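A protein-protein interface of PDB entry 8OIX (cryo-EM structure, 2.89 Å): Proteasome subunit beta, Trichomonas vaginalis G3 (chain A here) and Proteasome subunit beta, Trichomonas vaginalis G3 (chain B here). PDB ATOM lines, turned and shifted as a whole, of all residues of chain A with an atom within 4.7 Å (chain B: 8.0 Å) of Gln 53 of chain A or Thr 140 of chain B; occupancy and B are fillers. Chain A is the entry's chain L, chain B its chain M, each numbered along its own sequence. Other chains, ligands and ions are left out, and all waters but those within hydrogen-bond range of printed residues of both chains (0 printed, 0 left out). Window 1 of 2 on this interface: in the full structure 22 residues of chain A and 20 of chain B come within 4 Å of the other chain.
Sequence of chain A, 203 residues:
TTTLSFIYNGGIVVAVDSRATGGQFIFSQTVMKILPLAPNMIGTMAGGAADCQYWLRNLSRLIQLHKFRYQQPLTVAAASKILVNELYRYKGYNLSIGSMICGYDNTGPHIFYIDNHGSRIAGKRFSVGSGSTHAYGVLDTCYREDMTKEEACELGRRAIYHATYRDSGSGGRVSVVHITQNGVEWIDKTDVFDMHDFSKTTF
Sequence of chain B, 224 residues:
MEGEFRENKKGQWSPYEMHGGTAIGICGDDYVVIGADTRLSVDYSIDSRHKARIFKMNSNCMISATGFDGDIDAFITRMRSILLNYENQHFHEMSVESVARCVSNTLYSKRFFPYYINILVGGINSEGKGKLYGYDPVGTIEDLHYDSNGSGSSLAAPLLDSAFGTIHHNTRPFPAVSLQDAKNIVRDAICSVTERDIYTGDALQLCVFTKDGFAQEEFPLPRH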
ATOM      1  N   MET A  32     -16.393  12.101 -26.118  1.00  0.00           N
ATOM      2  CA  MET A  32     -15.749  10.817 -26.371  1.00  0.00           C
ATOM      3  C   MET A  32     -16.686   9.963 -27.216  1.00  0.00           C
ATOM      4  O   MET A  32     -17.734   9.517 -26.738  1.00  0.00           O
ATOM      5  CB  MET A  32     -15.397  10.117 -25.062  1.00  0.00           C
ATOM      6  CG  MET A  32     -14.760   8.753 -25.259  1.00  0.00           C
ATOM      7  SD  MET A  32     -13.372   8.792 -26.411  1.00  0.00           S
ATOM      8  CE  MET A  32     -12.256   9.902 -25.559  1.00  0.00           C
ATOM      9  N   LEU A  35     -16.665   4.271 -27.166  1.00  0.00           N
ATOM     10  CA  LEU A  35     -17.030   3.697 -25.884  1.00  0.00           C
ATOM     11  C   LEU A  35     -16.561   2.254 -25.852  1.00  0.00           C
ATOM     12  O   LEU A  35     -16.979   1.459 -26.708  1.00  0.00           O
ATOM     13  CB  LEU A  35     -18.539   3.776 -25.643  1.00  0.00           C
ATOM     14  CG  LEU A  35     -19.224   5.142 -25.505  1.00  0.00           C
ATOM     15  CD1 LEU A  35     -19.325   5.903 -26.825  1.00  0.00           C
ATOM     16  CD2 LEU A  35     -20.596   4.972 -24.877  1.00  0.00           C
ATOM     17  N   MET A  45     -19.493   6.113 -31.561  1.00  0.00           N
ATOM     18  CA  MET A  45     -20.721   6.866 -31.358  1.00  0.00           C
ATOM     19  C   MET A  45     -20.849   7.920 -32.452  1.00  0.00           C
ATOM     20  O   MET A  45     -19.977   8.785 -32.594  1.00  0.00           O
ATOM     21  CB  MET A  45     -20.727   7.469 -29.953  1.00  0.00           C
ATOM     22  CG  MET A  45     -21.285   8.857 -29.798  1.00  0.00           C
ATOM     23  SD  MET A  45     -20.895   9.405 -28.129  1.00  0.00           S
ATOM     24  CE  MET A  45     -21.674  11.003 -28.110  1.00  0.00           C
ATOM     25  N   ALA A  49     -26.249  11.491 -29.692  1.00  0.00           N
ATOM     26  CA  ALA A  49     -25.238  11.272 -28.665  1.00  0.00           C
ATOM     27  C   ALA A  49     -25.784  10.442 -27.511  1.00  0.00           C
ATOM     28  O   ALA A  49     -25.159   9.463 -27.084  1.00  0.00           O
ATOM     29  CB  ALA A  49     -24.720  12.619 -28.167  1.00  0.00           C
ATOM     30  N   ALA A  50     -26.959  10.815 -27.000  1.00  0.00           N
ATOM     31  CA  ALA A  50     -27.567  10.071 -25.904  1.00  0.00           C
ATOM     32  C   ALA A  50     -27.862   8.640 -26.317  1.00  0.00           C
ATOM     33  O   ALA A  50     -27.613   7.698 -25.556  1.00  0.00           O
ATOM     34  CB  ALA A  50     -28.844  10.766 -25.441  1.00  0.00           C
ATOM     35  N   ASP A  51     -28.411   8.461 -27.519  1.00  0.00           N
ATOM     36  CA  ASP A  51     -28.753   7.125 -27.984  1.00  0.00           C
ATOM     37  C   ASP A  51     -27.512   6.252 -28.079  1.00  0.00           C
ATOM     38  O   ASP A  51     -27.495   5.119 -27.587  1.00  0.00           O
ATOM     39  CB  ASP A  51     -29.451   7.214 -29.339  1.00  0.00           C
ATOM     40  CG  ASP A  51     -30.578   8.219 -29.346  1.00  0.00           C
ATOM     41  OD1 ASP A  51     -31.282   8.324 -28.324  1.00  0.00           O
ATOM     42  OD2 ASP A  51     -30.760   8.905 -30.372  1.00  0.00           O
ATOM     43  N   CYS A  52     -26.451   6.776 -28.695  1.00  0.00           N
ATOM     44  CA  CYS A  52     -25.235   5.989 -28.850  1.00  0.00           C
ATOM     45  C   CYS A  52     -24.611   5.669 -27.502  1.00  0.00           C
ATOM     46  O   CYS A  52     -24.177   4.539 -27.271  1.00  0.00           O
ATOM     47  CB  CYS A  52     -24.238   6.720 -29.740  1.00  0.00           C
ATOM     48  SG  CYS A  52     -24.638   6.610 -31.478  1.00  0.00           S
ATOM     49  N   GLN A  53     -24.630   6.623 -26.570  1.00  0.00           N
ATOM     50  CA  GLN A  53     -23.974   6.367 -25.294  1.00  0.00           C
ATOM     51  C   GLN A  53     -24.764   5.371 -24.459  1.00  0.00           C
ATOM     52  O   GLN A  53     -24.186   4.425 -23.904  1.00  0.00           O
ATOM     53  CB  GLN A  53     -23.805   7.676 -24.523  1.00  0.00           C
ATOM     54  CG  GLN A  53     -22.691   8.566 -25.026  1.00  0.00           C
ATOM     55  CD  GLN A  53     -22.551   9.823 -24.200  1.00  0.00           C
ATOM     56  OE1 GLN A  53     -23.355  10.080 -23.307  1.00  0.00           O
ATOM     57  NE2 GLN A  53     -21.527  10.615 -24.492  1.00  0.00           N
ATOM     58  N   TYR A  54     -26.089   5.515 -24.432  1.00  0.00           N
ATOM     59  CA  TYR A  54     -26.918   4.587 -23.677  1.00  0.00           C
ATOM     60  C   TYR A  54     -26.838   3.189 -24.267  1.00  0.00           C
ATOM     61  O   TYR A  54     -26.662   2.212 -23.536  1.00  0.00           O
ATOM     62  CB  TYR A  54     -28.367   5.072 -23.644  1.00  0.00           C
ATOM     63  CG  TYR A  54     -29.301   4.160 -22.878  1.00  0.00           C
ATOM     64  CD1 TYR A  54     -29.899   3.065 -23.491  1.00  0.00           C
ATOM     65  CD2 TYR A  54     -29.592   4.400 -21.544  1.00  0.00           C
ATOM     66  CE1 TYR A  54     -30.751   2.236 -22.796  1.00  0.00           C
ATOM     67  CE2 TYR A  54     -30.448   3.579 -20.843  1.00  0.00           C
ATOM     68  CZ  TYR A  54     -31.023   2.497 -21.474  1.00  0.00           C
ATOM     69  OH  TYR A  54     -31.874   1.673 -20.776  1.00  0.00           O
ATOM     70  N   TRP A  55     -26.963   3.069 -25.588  1.00  0.00           N
ATOM     71  CA  TRP A  55     -26.996   1.742 -26.176  1.00  0.00           C
ATOM     72  C   TRP A  55     -25.624   1.092 -26.225  1.00  0.00           C
ATOM     73  O   TRP A  55     -25.541  -0.134 -26.162  1.00  0.00           O
ATOM     74  CB  TRP A  55     -27.629   1.799 -27.565  1.00  0.00           C
ATOM     75  CG  TRP A  55     -29.094   2.056 -27.471  1.00  0.00           C
ATOM     76  CD1 TRP A  55     -29.750   3.205 -27.795  1.00  0.00           C
ATOM     77  CD2 TRP A  55     -30.083   1.159 -26.963  1.00  0.00           C
ATOM     78  NE1 TRP A  55     -31.093   3.068 -27.546  1.00  0.00           N
ATOM     79  CE2 TRP A  55     -31.322   1.820 -27.032  1.00  0.00           C
ATOM     80  CE3 TRP A  55     -30.042  -0.148 -26.468  1.00  0.00           C
ATOM     81  CZ2 TRP A  55     -32.509   1.220 -26.625  1.00  0.00           C
ATOM     82  CZ3 TRP A  55     -31.218  -0.739 -26.065  1.00  0.00           C
ATOM     83  CH2 TRP A  55     -32.436  -0.058 -26.144  1.00  0.00           C
ATOM     84  N   LEU A  56     -24.543   1.872 -26.255  1.00  0.00           N
ATOM     85  CA  LEU A  56     -23.226   1.260 -26.199  1.00  0.00           C
ATOM     86  C   LEU A  56     -22.868   0.836 -24.782  1.00  0.00           C
ATOM     87  O   LEU A  56     -22.243  -0.212 -24.600  1.00  0.00           O
ATOM     88  CB  LEU A  56     -22.176   2.214 -26.763  1.00  0.00           C
ATOM     89  CG  LEU A  56     -22.167   2.294 -28.290  1.00  0.00           C
ATOM     90  CD1 LEU A  56     -21.198   3.357 -28.764  1.00  0.00           C
ATOM     91  CD2 LEU A  56     -21.828   0.942 -28.892  1.00  0.00           C
ATOM     92  N   ARG A  57     -23.306   1.580 -23.761  1.00  0.00           N
ATOM     93  CA  ARG A  57     -23.083   1.083 -22.409  1.00  0.00           C
ATOM     94  C   ARG A  57     -24.026  -0.071 -22.080  1.00  0.00           C
ATOM     95  O   ARG A  57     -23.659  -0.966 -21.313  1.00  0.00           O
ATOM     96  CB  ARG A  57     -23.218   2.217 -21.390  1.00  0.00           C
ATOM     97  CG  ARG A  57     -24.633   2.658 -21.097  1.00  0.00           C
ATOM     98  CD  ARG A  57     -24.700   3.463 -19.812  1.00  0.00           C
ATOM     99  NE  ARG A  57     -24.394   4.869 -20.039  1.00  0.00           N
ATOM    100  CZ  ARG A  57     -25.306   5.813 -20.221  1.00  0.00           C
ATOM    101  NH1 ARG A  57     -26.599   5.538 -20.200  1.00  0.00           N
ATOM    102  NH2 ARG A  57     -24.910   7.066 -20.431  1.00  0.00           N
ATOM    103  N   ALA B 100     -24.025  10.659 -11.792  1.00  0.00           N
ATOM    104  CA  ALA B 100     -23.956  11.069 -13.187  1.00  0.00           C
ATOM    105  C   ALA B 100     -24.485   9.979 -14.108  1.00  0.00           C
ATOM    106  O   ALA B 100     -25.270  10.250 -15.028  1.00  0.00           O
ATOM    107  CB  ALA B 100     -22.518  11.422 -13.550  1.00  0.00           C
ATOM    108  N   ARG B 101     -24.067   8.736 -13.873  1.00  0.00           N
ATOM    109  CA  ARG B 101     -24.582   7.629 -14.670  1.00  0.00           C
ATOM    110  C   ARG B 101     -26.083   7.475 -14.472  1.00  0.00           C
ATOM    111  O   ARG B 101     -26.825   7.211 -15.427  1.00  0.00           O
ATOM    112  CB  ARG B 101     -23.856   6.338 -14.306  1.00  0.00           C
ATOM    113  CG  ARG B 101     -24.392   5.120 -15.021  1.00  0.00           C
ATOM    114  CD  ARG B 101     -24.256   5.269 -16.523  1.00  0.00           C
ATOM    115  NE  ARG B 101     -22.859   5.306 -16.936  1.00  0.00           N
ATOM    116  CZ  ARG B 101     -22.118   4.230 -17.158  1.00  0.00           C
ATOM    117  NH1 ARG B 101     -22.604   3.010 -17.000  1.00  0.00           N
ATOM    118  NH2 ARG B 101     -20.855   4.381 -17.544  1.00  0.00           N
ATOM    119  N   VAL B 103     -28.184   9.856 -13.699  1.00  0.00           N
ATOM    120  CA  VAL B 103     -28.829  10.958 -14.408  1.00  0.00           C
ATOM    121  C   VAL B 103     -28.928  10.646 -15.890  1.00  0.00           C
ATOM    122  O   VAL B 103     -29.967  10.872 -16.521  1.00  0.00           O
ATOM    123  CB  VAL B 103     -28.067  12.273 -14.167  1.00  0.00           C
ATOM    124  CG1 VAL B 103     -28.496  13.327 -15.171  1.00  0.00           C
ATOM    125  CG2 VAL B 103     -28.306  12.767 -12.772  1.00  0.00           C
ATOM    126  N   SER B 104     -27.846  10.125 -16.471  1.00  0.00           N
ATOM    127  CA  SER B 104     -27.880   9.742 -17.877  1.00  0.00           C
ATOM    128  C   SER B 104     -28.981   8.719 -18.132  1.00  0.00           C
ATOM    129  O   SER B 104     -29.805   8.884 -19.040  1.00  0.00           O
ATOM    130  CB  SER B 104     -26.519   9.196 -18.303  1.00  0.00           C
ATOM    131  OG  SER B 104     -26.414   9.132 -19.714  1.00  0.00           O
ATOM    132  N   ASN B 105     -29.026   7.666 -17.314  1.00  0.00           N
ATOM    133  CA  ASN B 105     -30.018   6.616 -17.515  1.00  0.00           C
ATOM    134  C   ASN B 105     -31.433   7.100 -17.219  1.00  0.00           C
ATOM    135  O   ASN B 105     -32.378   6.680 -17.891  1.00  0.00           O
ATOM    136  CB  ASN B 105     -29.675   5.406 -16.650  1.00  0.00           C
ATOM    137  CG  ASN B 105     -28.385   4.740 -17.075  1.00  0.00           C
ATOM    138  OD1 ASN B 105     -28.090   4.636 -18.265  1.00  0.00           O
ATOM    139  ND2 ASN B 105     -27.603   4.295 -16.105  1.00  0.00           N
ATOM    140  N   LEU B 107     -32.596  10.273 -17.582  1.00  0.00           N
ATOM    141  CA  LEU B 107     -32.995  11.086 -18.723  1.00  0.00           C
ATOM    142  C   LEU B 107     -33.301  10.218 -19.934  1.00  0.00           C
ATOM    143  O   LEU B 107     -34.255  10.488 -20.672  1.00  0.00           O
ATOM    144  CB  LEU B 107     -31.903  12.102 -19.047  1.00  0.00           C
ATOM    145  CG  LEU B 107     -31.675  13.229 -18.042  1.00  0.00           C
ATOM    146  CD1 LEU B 107     -30.423  14.009 -18.397  1.00  0.00           C
ATOM    147  CD2 LEU B 107     -32.882  14.145 -18.007  1.00  0.00           C
ATOM    148  N   TYR B 108     -32.502   9.172 -20.163  1.00  0.00           N
ATOM    149  CA  TYR B 108     -32.737   8.335 -21.334  1.00  0.00           C
ATOM    150  C   TYR B 108     -33.965   7.449 -21.161  1.00  0.00           C
ATOM    151  O   TYR B 108     -34.572   7.044 -22.156  1.00  0.00           O
ATOM    152  CB  TYR B 108     -31.512   7.481 -21.647  1.00  0.00           C
ATOM    153  CG  TYR B 108     -31.546   6.944 -23.056  1.00  0.00           C
ATOM    154  CD1 TYR B 108     -31.029   7.686 -24.106  1.00  0.00           C
ATOM    155  CD2 TYR B 108     -32.130   5.720 -23.344  1.00  0.00           C
ATOM    156  CE1 TYR B 108     -31.070   7.213 -25.395  1.00  0.00           C
ATOM    157  CE2 TYR B 108     -32.174   5.239 -24.634  1.00  0.00           C
ATOM    158  CZ  TYR B 108     -31.641   5.989 -25.656  1.00  0.00           C
ATOM    159  OH  TYR B 108     -31.681   5.516 -26.944  1.00  0.00           O
ATOM    160  N   ARG B 111     -36.374   8.770 -23.168  1.00  0.00           N
ATOM    161  CA  ARG B 111     -35.810   9.152 -24.461  1.00  0.00           C
ATOM    162  C   ARG B 111     -36.888   9.553 -25.461  1.00  0.00           C
ATOM    163  O   ARG B 111     -36.670  10.446 -26.287  1.00  0.00           O
ATOM    164  CB  ARG B 111     -34.969   8.002 -25.022  1.00  0.00           C
ATOM    165  CG  ARG B 111     -34.532   8.159 -26.467  1.00  0.00           C
ATOM    166  CD  ARG B 111     -33.720   9.422 -26.678  1.00  0.00           C
ATOM    167  NE  ARG B 111     -33.275   9.549 -28.061  1.00  0.00           N
ATOM    168  CZ  ARG B 111     -34.027  10.002 -29.052  1.00  0.00           C
ATOM    169  NH1 ARG B 111     -35.276  10.391 -28.851  1.00  0.00           N
ATOM    170  NH2 ARG B 111     -33.515  10.070 -30.278  1.00  0.00           N
ATOM    171  N   ILE B 119     -28.890  19.205 -17.781  1.00  0.00           N
ATOM    172  CA  ILE B 119     -28.464  18.855 -16.432  1.00  0.00           C
ATOM    173  C   ILE B 119     -26.968  19.085 -16.289  1.00  0.00           C
ATOM    174  O   ILE B 119     -26.184  18.753 -17.186  1.00  0.00           O
ATOM    175  CB  ILE B 119     -28.816  17.389 -16.114  1.00  0.00           C
ATOM    176  CG1 ILE B 119     -30.321  17.162 -16.228  1.00  0.00           C
ATOM    177  CG2 ILE B 119     -28.338  17.009 -14.726  1.00  0.00           C
ATOM    178  CD1 ILE B 119     -31.110  17.893 -15.197  1.00  0.00           C
ATOM    179  N   TYR B 133     -20.577  16.969 -14.804  1.00  0.00           N
ATOM    180  CA  TYR B 133     -21.118  16.202 -15.918  1.00  0.00           C
ATOM    181  C   TYR B 133     -22.206  17.017 -16.596  1.00  0.00           C
ATOM    182  O   TYR B 133     -23.180  17.415 -15.948  1.00  0.00           O
ATOM    183  CB  TYR B 133     -21.674  14.860 -15.439  1.00  0.00           C
ATOM    184  CG  TYR B 133     -20.641  13.957 -14.809  1.00  0.00           C
ATOM    185  CD1 TYR B 133     -20.334  14.056 -13.459  1.00  0.00           C
ATOM    186  CD2 TYR B 133     -19.984  12.996 -15.561  1.00  0.00           C
ATOM    187  CE1 TYR B 133     -19.398  13.227 -12.880  1.00  0.00           C
ATOM    188  CE2 TYR B 133     -19.047  12.164 -14.991  1.00  0.00           C
ATOM    189  CZ  TYR B 133     -18.758  12.284 -13.651  1.00  0.00           C
ATOM    190  OH  TYR B 133     -17.822  11.452 -13.083  1.00  0.00           O
ATOM    191  N   GLY B 134     -22.034  17.264 -17.890  1.00  0.00           N
ATOM    192  CA  GLY B 134     -23.030  17.965 -18.672  1.00  0.00           C
ATOM    193  C   GLY B 134     -23.960  17.011 -19.401  1.00  0.00           C
ATOM    194  O   GLY B 134     -23.575  15.896 -19.772  1.00  0.00           O
ATOM    195  N   TYR B 135     -25.196  17.475 -19.605  1.00  0.00           N
ATOM    196  CA  TYR B 135     -26.246  16.665 -20.203  1.00  0.00           C
ATOM    197  C   TYR B 135     -27.058  17.466 -21.207  1.00  0.00           C
ATOM    198  O   TYR B 135     -27.152  18.693 -21.125  1.00  0.00           O
ATOM    199  CB  TYR B 135     -27.198  16.115 -19.140  1.00  0.00           C
ATOM    200  CG  TYR B 135     -26.545  15.123 -18.229  1.00  0.00           C
ATOM    201  CD1 TYR B 135     -25.896  15.538 -17.079  1.00  0.00           C
ATOM    202  CD2 TYR B 135     -26.570  13.771 -18.522  1.00  0.00           C
ATOM    203  CE1 TYR B 135     -25.292  14.636 -16.250  1.00  0.00           C
ATOM    204  CE2 TYR B 135     -25.972  12.865 -17.699  1.00  0.00           C
ATOM    205  CZ  TYR B 135     -25.334  13.303 -16.566  1.00  0.00           C
ATOM    206  OH  TYR B 135     -24.736  12.397 -15.745  1.00  0.00           O
ATOM    207  N   ASP B 136     -27.641  16.749 -22.153  1.00  0.00           N
ATOM    208  CA  ASP B 136     -28.716  17.231 -23.002  1.00  0.00           C
ATOM    209  C   ASP B 136     -30.043  16.667 -22.510  1.00  0.00           C
ATOM    210  O   ASP B 136     -30.073  15.800 -21.632  1.00  0.00           O
ATOM    211  CB  ASP B 136     -28.447  16.840 -24.463  1.00  0.00           C
ATOM    212  CG  ASP B 136     -28.405  15.340 -24.686  1.00  0.00           C
ATOM    213  OD1 ASP B 136     -28.658  14.562 -23.742  1.00  0.00           O
ATOM    214  OD2 ASP B 136     -28.116  14.931 -25.829  1.00  0.00           O
ATOM    215  N   PRO B 137     -31.175  17.155 -23.030  1.00  0.00           N
ATOM    216  CA  PRO B 137     -32.466  16.650 -22.534  1.00  0.00           C
ATOM    217  C   PRO B 137     -32.638  15.146 -22.666  1.00  0.00           C
ATOM    218  O   PRO B 137     -33.326  14.539 -21.837  1.00  0.00           O
ATOM    219  CB  PRO B 137     -33.485  17.414 -23.390  1.00  0.00           C
ATOM    220  CG  PRO B 137     -32.798  18.676 -23.726  1.00  0.00           C
ATOM    221  CD  PRO B 137     -31.357  18.317 -23.918  1.00  0.00           C
ATOM    222  N   VAL B 138     -32.027  14.517 -23.677  1.00  0.00           N
ATOM    223  CA  VAL B 138     -32.218  13.088 -23.906  1.00  0.00           C
ATOM    224  C   VAL B 138     -31.199  12.225 -23.175  1.00  0.00           C
ATOM    225  O   VAL B 138     -31.214  10.998 -23.337  1.00  0.00           O
ATOM    226  CB  VAL B 138     -32.197  12.770 -25.415  1.00  0.00           C
ATOM    227  CG1 VAL B 138     -33.502  13.201 -26.056  1.00  0.00           C
ATOM    228  CG2 VAL B 138     -31.036  13.475 -26.082  1.00  0.00           C
ATOM    229  N   GLY B 139     -30.327  12.817 -22.365  1.00  0.00           N
ATOM    230  CA  GLY B 139     -29.473  12.055 -21.478  1.00  0.00           C
ATOM    231  C   GLY B 139     -28.043  11.816 -21.905  1.00  0.00           C
ATOM    232  O   GLY B 139     -27.392  10.939 -21.328  1.00  0.00           O
ATOM    233  N   THR B 140     -27.533  12.545 -22.896  1.00  0.00           N
ATOM    234  CA  THR B 140     -26.108  12.469 -23.192  1.00  0.00           C
ATOM    235  C   THR B 140     -25.308  12.906 -21.977  1.00  0.00           C
ATOM    236  O   THR B 140     -25.546  13.979 -21.420  1.00  0.00           O
ATOM    237  CB  THR B 140     -25.742  13.356 -24.379  1.00  0.00           C
ATOM    238  OG1 THR B 140     -26.523  12.993 -25.522  1.00  0.00           O
ATOM    239  CG2 THR B 140     -24.264  13.222 -24.704  1.00  0.00           C
ATOM    240  N   ILE B 141     -24.350  12.087 -21.574  1.00  0.00           N
ATOM    241  CA  ILE B 141     -23.508  12.398 -20.430  1.00  0.00           C
ATOM    242  C   ILE B 141     -22.147  12.808 -20.961  1.00  0.00           C
ATOM    243  O   ILE B 141     -21.673  12.288 -21.978  1.00  0.00           O
ATOM    244  CB  ILE B 141     -23.391  11.203 -19.458  1.00  0.00           C
ATOM    245  CG1 ILE B 141     -22.597  11.590 -18.209  1.00  0.00           C
ATOM    246  CG2 ILE B 141     -22.762  10.002 -20.143  1.00  0.00           C
ATOM    247  CD1 ILE B 141     -22.575  10.513 -17.151  1.00  0.00           C
ATOM    248  N   GLU B 142     -21.520  13.766 -20.284  1.00  0.00           N
ATOM    249  CA  GLU B 142     -20.183  14.172 -20.700  1.00  0.00           C
ATOM    250  C   GLU B 142     -19.429  14.711 -19.498  1.00  0.00           C
ATOM    251  O   GLU B 142     -19.833  15.720 -18.917  1.00  0.00           O
ATOM    252  CB  GLU B 142     -20.252  15.217 -21.811  1.00  0.00           C
ATOM    253  CG  GLU B 142     -18.906  15.578 -22.393  1.00  0.00           C
ATOM    254  CD  GLU B 142     -19.005  16.653 -23.448  1.00  0.00           C
ATOM    255  OE1 GLU B 142     -20.138  17.070 -23.768  1.00  0.00           O
ATOM    256  OE2 GLU B 142     -17.950  17.075 -23.965  1.00  0.00           O
ATOM    257  N   ASP B 143     -18.342  14.037 -19.129  1.00  0.00           N
ATOM    258  CA  ASP B 143     -17.484  14.514 -18.050  1.00  0.00           C
ATOM    259  C   ASP B 143     -16.737  15.749 -18.530  1.00  0.00           C
ATOM    260  O   ASP B 143     -15.867  15.662 -19.401  1.00  0.00           O
ATOM    261  CB  ASP B 143     -16.518  13.414 -17.620  1.00  0.00           C
ATOM    262  CG  ASP B 143     -15.840  13.715 -16.297  1.00  0.00           C
ATOM    263  OD1 ASP B 143     -16.012  14.835 -15.776  1.00  0.00           O
ATOM    264  OD2 ASP B 143     -15.135  12.826 -15.776  1.00  0.00           O
ATOM    265  N   LEU B 144     -17.075  16.900 -17.961  1.00  0.00           N
ATOM    266  CA  LEU B 144     -16.638  18.194 -18.451  1.00  0.00           C
ATOM    267  C   LEU B 144     -15.902  18.955 -17.360  1.00  0.00           C
ATOM    268  O   LEU B 144     -16.200  18.815 -16.170  1.00  0.00           O
ATOM    269  CB  LEU B 144     -17.829  19.019 -18.940  1.00  0.00           C
ATOM    270  CG  LEU B 144     -18.423  18.528 -20.254  1.00  0.00           C
ATOM    271  CD1 LEU B 144     -19.750  19.192 -20.527  1.00  0.00           C
ATOM    272  CD2 LEU B 144     -17.439  18.828 -21.365  1.00  0.00           C
ATOM    273  N   ASP B 147     -19.263  23.638 -18.342  1.00  0.00           N
ATOM    274  CA  ASP B 147     -20.394  23.503 -19.246  1.00  0.00           C
ATOM    275  C   ASP B 147     -21.348  24.660 -19.011  1.00  0.00           C
ATOM    276  O   ASP B 147     -21.326  25.307 -17.962  1.00  0.00           O
ATOM    277  CB  ASP B 147     -21.114  22.165 -19.062  1.00  0.00           C
ATOM    278  CG  ASP B 147     -21.983  21.802 -20.251  1.00  0.00           C
ATOM    279  OD1 ASP B 147     -21.653  22.223 -21.381  1.00  0.00           O
ATOM    280  OD2 ASP B 147     -22.992  21.092 -20.060  1.00  0.00           O
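Of chain B, only Thr 140 (3.6 Å) and Ile 141 (2.8 Å) come within 4 Å of Gln 53 of chain A.
Of the printed residues of chain A, Thr 140 of chain B touches Ala 49 (3.2 Å), Ala 50 (2.7 Å) and Gln 53 (3.6 Å).
Ala 50 of chain A touches just these residues of chain B: Tyr 108, Val 138, Gly 139 and Thr 140.
Of the printed residues of chain B, Trp 55 of chain A touches Tyr 108.
Of the printed residues of chain A, Val 138 of chain B touches Ala 50 (3.2 Å).
Printed residues of chain B within 4 Å of Tyr 54 of chain A: Asn 105 (3.6 Å) and Tyr 108 (3.3 Å).
Of the printed residues of chain B, Ala 49 of chain A touches Thr 140.
Of the printed residues of chain A, Ile 141 of chain B touches Gln 53 and Arg 57.
The side-chain hydroxyl (OG1) of Thr 140 of chain B lies within hydrogen-bond range of the backbone NH (N) of Ala 50 of chain A (2.7 Å).
The side-chain carboxylate (OD1) of Asp 51 of chain A lies close to the side-chain hydroxyl (OH) of Tyr 108 of chain B, at 3.2 Å.
The side-chain carboxylate (OD2) of Asp 51 of chain A is in salt-bridge range of the guanidinium group (NH2) of Arg 111 of chain B (3.0 Å).
OE1 of Gln 53 of chain A lies within hydrogen-bond range of N of Ile 141 of chain B (2.8 Å).
The indole nitrogen of Trp 55 of chain A is in hydrogen-bond range of the side-chain hydroxyl of Tyr 108 of chain B (2.6 Å).
NH2 of Arg 57 of chain A is in hydrogen-bond range of OG of Ser 104 of chain B, at 2.7 Å.
The guanidinium group of Arg 57 of chain A sits at hydrogen-bond distance from the side-chain amide oxygen of Asn 105 of chain B (2.6 Å).
The guanidinium group (NE) of Arg 101 of chain B lies close to the guanidinium group (NE) of Arg 57 of chain A, at 3.5 Å.
Of the 22 printed residues of chain B, 9 touch a printed residue of chain A.
Among the printed residues, 16 pairs touch across the chains.
Among the printed residues, Asp or Glu carboxylates within 4 Å of a Lys or Arg side-chain nitrogen of the other chain: Asp 51 of chain A with Arg 111 of chain B.
OG1 of Thr 140 of chain B touches CB of Ala 49 of chain A, at 3.2 Å.
O of Ala 50 of chain A touches CE1 of Tyr 108 of chain B, at 3.5 Å.
Val 138 of chain B touches Ala 50 of chain A.
Gly 139 of chain B touches Ala 50 of chain A.
OE1 of Gln 53 of chain A touches CG2 of Thr 140 of chain B, at 3.6 Å.
Asn 105 of chain B touches Tyr 54 of chain A (OD1 to CD2, 3.6 Å).
Tyr 54 of chain A touches Tyr 108 of chain B (CG to CD2, 3.3 Å).
CG2 of Ile 141 of chain B touches NH2 of Arg 57 of chain A (3.6 Å).
The side-chain amide nitrogen (ND2) of Asn 105 of chain B lies within hydrogen-bond range of the backbone carbonyl oxygen (O) of Arg 101 of chain B (3.1 Å).
O of Gly 139 of chain B lies within hydrogen-bond range of OG of Ser 104 of chain B, at 2.6 Å.
N of Val 138 of chain B sits close to OD1 of Asp 136 of chain B (3.4 Å).
OD1 of Asp 136 of chain B sits at hydrogen-bond distance from N of Gly 139 of chain B (2.8 Å).
N of Thr 140 of chain B is in hydrogen-bond range of OD1 of Asp 136 of chain B (2.5 Å).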
